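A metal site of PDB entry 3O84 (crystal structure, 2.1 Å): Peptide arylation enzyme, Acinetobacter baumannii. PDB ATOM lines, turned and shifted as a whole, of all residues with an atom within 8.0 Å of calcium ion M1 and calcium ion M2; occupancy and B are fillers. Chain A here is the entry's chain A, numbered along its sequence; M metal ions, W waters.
The backbone NH (N) of Leu 309 lies within hydrogen-bond range of the backbone carbonyl oxygen (O) of Val 282 (3.4 Å).
OD1 of Asn 332 lies close to O of Val 330 (3.5 Å).
The backbone carbonyl oxygen of Val 327 lies within hydrogen-bond range of the backbone NH of Asn 332, 3.3 Å away.
OE1 of Gln 307 lies close to O of Lys 303 (3.0 Å).
Within 4 Å of calcium ion M1: Gln 307, Leu 309 and Asn 332.
Residues that only touch calcium ion M2: Pro 328.
Within 4 Å of calcium ion M2: Pro 328, Glu 329 and Asn 332.
Along chain A the residues within 4 Å of calcium ion M2 span positions 328 to 332.
Calcium ion M1 is bound by the backbone carbonyl oxygen of Gln 307 (2.3 Å), the backbone carbonyl oxygen of Asn 332 (2.3 Å), the backbone carbonyl oxygen of Leu 309 (2.4 Å), water W4 (2.4 Å) and water W1 (2.4 Å).
Calcium ion M1 has five donor atoms within binding distance.
Calcium ion M2 is bound by water W5, at 2.3 Å.
O of Glu 329 binds calcium ion M2 (2.4 Å).
The side-chain amide oxygen (OD1) of Asn 332 is bound to calcium ion M2 (2.4 Å).
Calcium ion M2 is bound by water W2 (2.4 Å).
Calcium ion M2 is bound by water W3 (2.5 Å).
Water W1 lies within hydrogen-bond range of the backbone carbonyl oxygen (O) of Leu 331 and the backbone carbonyl oxygen (O) of Ile 306.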
ATOM      1  N   VAL A 282      27.148  19.271  11.362  1.00  0.00           N
ATOM      2  CA  VAL A 282      27.610  20.533  10.773  1.00  0.00           C
ATOM      3  C   VAL A 282      28.231  21.386  11.887  1.00  0.00           C
ATOM      4  O   VAL A 282      27.670  21.505  12.987  1.00  0.00           O
ATOM      5  CB  VAL A 282      26.441  21.282  10.117  1.00  0.00           C
ATOM      6  CG1 VAL A 282      26.835  22.690   9.684  1.00  0.00           C
ATOM      7  CG2 VAL A 282      25.877  20.474   8.925  1.00  0.00           C
ATOM      8  N   ASN A 283      29.416  21.950  11.620  1.00  0.00           N
ATOM      9  CA  ASN A 283      30.083  22.796  12.611  1.00  0.00           C
ATOM     10  C   ASN A 283      30.245  24.260  12.213  1.00  0.00           C
ATOM     11  O   ASN A 283      30.747  25.068  12.994  1.00  0.00           O
ATOM     12  CB  ASN A 283      31.421  22.188  13.063  1.00  0.00           C
ATOM     13  CG  ASN A 283      32.319  21.800  11.896  1.00  0.00           C
ATOM     14  OD1 ASN A 283      32.351  22.470  10.846  1.00  0.00           O
ATOM     15  ND2 ASN A 283      33.069  20.716  12.071  1.00  0.00           N
ATOM     16  N   LYS A 303      17.721  23.119  20.775  1.00  0.00           N
ATOM     17  CA  LYS A 303      19.086  23.278  21.259  1.00  0.00           C
ATOM     18  C   LYS A 303      19.958  22.033  21.006  1.00  0.00           C
ATOM     19  O   LYS A 303      21.100  22.172  20.553  1.00  0.00           O
ATOM     20  CB  LYS A 303      19.041  23.695  22.746  1.00  0.00           C
ATOM     21  CG  LYS A 303      20.243  23.306  23.601  1.00  0.00           C
ATOM     22  CD  LYS A 303      19.989  23.514  25.104  1.00  0.00           C
ATOM     23  CE  LYS A 303      19.246  22.315  25.761  1.00  0.00           C
ATOM     24  NZ  LYS A 303      20.077  21.064  25.905  1.00  0.00           N
ATOM     25  N   ILE A 306      21.412  21.511  17.214  1.00  0.00           N
ATOM     26  CA  ILE A 306      22.377  22.463  16.652  1.00  0.00           C
ATOM     27  C   ILE A 306      23.638  22.656  17.489  1.00  0.00           C
ATOM     28  O   ILE A 306      24.462  23.522  17.180  1.00  0.00           O
ATOM     29  CB  ILE A 306      21.734  23.838  16.399  1.00  0.00           C
ATOM     30  CG1 ILE A 306      21.296  24.473  17.719  1.00  0.00           C
ATOM     31  CG2 ILE A 306      20.563  23.683  15.446  1.00  0.00           C
ATOM     32  CD1 ILE A 306      21.043  25.970  17.627  1.00  0.00           C
ATOM     33  N   GLN A 307      23.794  21.853  18.545  1.00  0.00           N
ATOM     34  CA  GLN A 307      24.956  22.002  19.438  1.00  0.00           C
ATOM     35  C   GLN A 307      26.312  21.991  18.735  1.00  0.00           C
ATOM     36  O   GLN A 307      27.215  22.760  19.111  1.00  0.00           O
ATOM     37  CB  GLN A 307      24.907  20.993  20.598  1.00  0.00           C
ATOM     38  CG  GLN A 307      24.026  21.470  21.785  1.00  0.00           C
ATOM     39  CD  GLN A 307      24.187  22.982  22.094  1.00  0.00           C
ATOM     40  OE1 GLN A 307      23.336  23.813  21.740  1.00  0.00           O
ATOM     41  NE2 GLN A 307      25.305  23.334  22.704  1.00  0.00           N
ATOM     42  N   SER A 308      26.424  21.161  17.693  1.00  0.00           N
ATOM     43  CA  SER A 308      27.682  20.970  16.936  1.00  0.00           C
ATOM     44  C   SER A 308      28.160  22.222  16.190  1.00  0.00           C
ATOM     45  O   SER A 308      29.328  22.276  15.820  1.00  0.00           O
ATOM     46  CB  SER A 308      27.598  19.754  15.980  1.00  0.00           C
ATOM     47  OG  SER A 308      26.653  19.963  14.922  1.00  0.00           O
ATOM     48  N   LEU A 309      27.279  23.200  15.956  1.00  0.00           N
ATOM     49  CA  LEU A 309      27.704  24.462  15.338  1.00  0.00           C
ATOM     50  C   LEU A 309      28.803  25.105  16.158  1.00  0.00           C
ATOM     51  O   LEU A 309      28.628  25.305  17.350  1.00  0.00           O
ATOM     52  CB  LEU A 309      26.535  25.471  15.226  1.00  0.00           C
ATOM     53  CG  LEU A 309      25.504  25.282  14.115  1.00  0.00           C
ATOM     54  CD1 LEU A 309      24.416  26.329  14.239  1.00  0.00           C
ATOM     55  CD2 LEU A 309      26.178  25.346  12.738  1.00  0.00           C
ATOM     56  N   LYS A 310      29.921  25.436  15.534  1.00  0.00           N
ATOM     57  CA  LYS A 310      31.013  26.103  16.254  1.00  0.00           C
ATOM     58  C   LYS A 310      31.158  27.532  15.797  1.00  0.00           C
ATOM     59  O   LYS A 310      31.653  28.376  16.523  1.00  0.00           O
ATOM     60  CB  LYS A 310      32.345  25.376  16.031  1.00  0.00           C
ATOM     61  CG  LYS A 310      32.427  23.973  16.615  1.00  0.00           C
ATOM     62  CD  LYS A 310      33.783  23.347  16.285  1.00  0.00           C
ATOM     63  CE  LYS A 310      34.024  22.064  17.071  1.00  0.00           C
ATOM     64  NZ  LYS A 310      35.400  21.533  16.778  1.00  0.00           N
ATOM     65  N   LEU A 311      30.767  27.810  14.550  1.00  0.00           N
ATOM     66  CA  LEU A 311      30.957  29.145  14.005  1.00  0.00           C
ATOM     67  C   LEU A 311      29.788  29.486  13.093  1.00  0.00           C
ATOM     68  O   LEU A 311      29.409  28.681  12.234  1.00  0.00           O
ATOM     69  CB  LEU A 311      32.299  29.239  13.260  1.00  0.00           C
ATOM     70  CG  LEU A 311      32.654  30.527  12.508  1.00  0.00           C
ATOM     71  CD1 LEU A 311      32.883  31.672  13.478  1.00  0.00           C
ATOM     72  CD2 LEU A 311      33.892  30.320  11.601  1.00  0.00           C
ATOM     73  N   GLN A 326      22.825  37.742  20.700  1.00  0.00           N
ATOM     74  CA  GLN A 326      21.986  36.551  20.818  1.00  0.00           C
ATOM     75  C   GLN A 326      22.560  35.322  20.118  1.00  0.00           C
ATOM     76  O   GLN A 326      22.157  34.194  20.414  1.00  0.00           O
ATOM     77  CB  GLN A 326      20.574  36.803  20.299  1.00  0.00           C
ATOM     78  CG  GLN A 326      19.769  37.771  21.157  1.00  0.00           C
ATOM     79  CD  GLN A 326      18.331  37.829  20.712  1.00  0.00           C
ATOM     80  OE1 GLN A 326      17.612  36.824  20.744  1.00  0.00           O
ATOM     81  NE2 GLN A 326      17.883  39.022  20.296  1.00  0.00           N
ATOM     82  N   VAL A 327      23.478  35.511  19.164  1.00  0.00           N
ATOM     83  CA  VAL A 327      24.045  34.358  18.441  1.00  0.00           C
ATOM     84  C   VAL A 327      24.792  33.387  19.397  1.00  0.00           C
ATOM     85  O   VAL A 327      24.416  32.222  19.477  1.00  0.00           O
ATOM     86  CB  VAL A 327      24.902  34.779  17.205  1.00  0.00           C
ATOM     87  CG1 VAL A 327      25.713  33.587  16.656  1.00  0.00           C
ATOM     88  CG2 VAL A 327      24.008  35.372  16.128  1.00  0.00           C
ATOM     89  N   PRO A 328      25.822  33.867  20.127  1.00  0.00           N
ATOM     90  CA  PRO A 328      26.464  32.938  21.067  1.00  0.00           C
ATOM     91  C   PRO A 328      25.561  32.544  22.219  1.00  0.00           C
ATOM     92  O   PRO A 328      25.631  31.406  22.684  1.00  0.00           O
ATOM     93  CB  PRO A 328      27.685  33.710  21.578  1.00  0.00           C
ATOM     94  CG  PRO A 328      27.415  35.132  21.279  1.00  0.00           C
ATOM     95  CD  PRO A 328      26.563  35.136  20.021  1.00  0.00           C
ATOM     96  N   GLU A 329      24.701  33.465  22.663  1.00  0.00           N
ATOM     97  CA  GLU A 329      23.749  33.197  23.753  1.00  0.00           C
ATOM     98  C   GLU A 329      22.748  32.084  23.421  1.00  0.00           C
ATOM     99  O   GLU A 329      22.493  31.212  24.267  1.00  0.00           O
ATOM    100  CB  GLU A 329      23.024  34.489  24.156  1.00  0.00           C
ATOM    101  CG  GLU A 329      22.082  34.352  25.358  1.00  0.00           C
ATOM    102  CD  GLU A 329      22.837  34.122  26.680  1.00  0.00           C
ATOM    103  OE1 GLU A 329      23.905  34.726  26.881  1.00  0.00           O
ATOM    104  OE2 GLU A 329      22.341  33.323  27.509  1.00  0.00           O
ATOM    105  N   VAL A 330      22.192  32.106  22.215  1.00  0.00           N
ATOM    106  CA  VAL A 330      21.078  31.220  21.851  1.00  0.00           C
ATOM    107  C   VAL A 330      21.470  30.090  20.865  1.00  0.00           C
ATOM    108  O   VAL A 330      20.969  28.967  20.969  1.00  0.00           O
ATOM    109  CB  VAL A 330      19.862  32.048  21.303  1.00  0.00           C
ATOM    110  CG1 VAL A 330      18.749  31.158  20.793  1.00  0.00           C
ATOM    111  CG2 VAL A 330      19.328  33.014  22.373  1.00  0.00           C
ATOM    112  N   LEU A 331      22.331  30.386  19.898  1.00  0.00           N
ATOM    113  CA  LEU A 331      22.740  29.370  18.922  1.00  0.00           C
ATOM    114  C   LEU A 331      23.998  28.632  19.371  1.00  0.00           C
ATOM    115  O   LEU A 331      24.449  27.684  18.737  1.00  0.00           O
ATOM    116  CB  LEU A 331      22.903  29.982  17.515  1.00  0.00           C
ATOM    117  CG  LEU A 331      21.656  30.662  16.886  1.00  0.00           C
ATOM    118  CD1 LEU A 331      21.957  31.310  15.539  1.00  0.00           C
ATOM    119  CD2 LEU A 331      20.516  29.655  16.735  1.00  0.00           C
ATOM    120  N   ASN A 332      24.574  29.104  20.477  1.00  0.00           N
ATOM    121  CA  ASN A 332      25.637  28.382  21.188  1.00  0.00           C
ATOM    122  C   ASN A 332      26.858  28.145  20.303  1.00  0.00           C
ATOM    123  O   ASN A 332      27.403  27.048  20.242  1.00  0.00           O
ATOM    124  CB  ASN A 332      25.065  27.072  21.772  1.00  0.00           C
ATOM    125  CG  ASN A 332      23.883  27.311  22.723  1.00  0.00           C
ATOM    126  OD1 ASN A 332      23.636  28.446  23.128  1.00  0.00           O
ATOM    127  ND2 ASN A 332      23.154  26.273  23.053  1.00  0.00           N
ATOM    128  N   CYS A 333      27.269  29.194  19.602  1.00  0.00           N
ATOM    129  CA  CYS A 333      28.413  29.119  18.705  1.00  0.00           C
ATOM    130  C   CYS A 333      29.031  30.511  18.611  1.00  0.00           C
ATOM    131  O   CYS A 333      28.394  31.503  18.961  1.00  0.00           O
ATOM    132  CB  CYS A 333      27.990  28.608  17.328  1.00  0.00           C
ATOM    133  SG  CYS A 333      26.786  29.695  16.529  1.00  0.00           S
ATOM    134  N   LYS A 334      30.275  30.561  18.139  1.00  0.00           N
ATOM    135  CA  LYS A 334      30.963  31.821  17.920  1.00  0.00           C
ATOM    136  C   LYS A 334      30.316  32.564  16.748  1.00  0.00           C
ATOM    137  O   LYS A 334      29.844  31.945  15.798  1.00  0.00           O
ATOM    138  CB  LYS A 334      32.459  31.541  17.663  1.00  0.00           C
ATOM    139  CG  LYS A 334      33.264  32.650  16.971  1.00  0.00           C
ATOM    140  CD  LYS A 334      33.519  33.875  17.875  1.00  0.00           C
ATOM    141  CE  LYS A 334      34.733  33.691  18.798  1.00  0.00           C
ATOM    142  NZ  LYS A 334      34.773  34.777  19.833  1.00  0.00           N
HETATM  143 CA    CA M   1      27.945  24.870  19.589  1.00  0.00          CA
HETATM  144 CA    CA M   2      23.541  29.379  25.344  1.00  0.00          CA
HETATM  145  O   HOH W   1      25.707  25.338  18.804  1.00  0.00           O
HETATM  146  O   HOH W   2      25.858  30.081  25.210  1.00  0.00           O
HETATM  147  O   HOH W   3      23.947  30.489  27.575  1.00  0.00           O
HETATM  148  O   HOH W   4      27.492  24.265  21.854  1.00  0.00           O
HETATM  149  O   HOH W   5      21.490  28.447  25.438  1.00  0.00           O
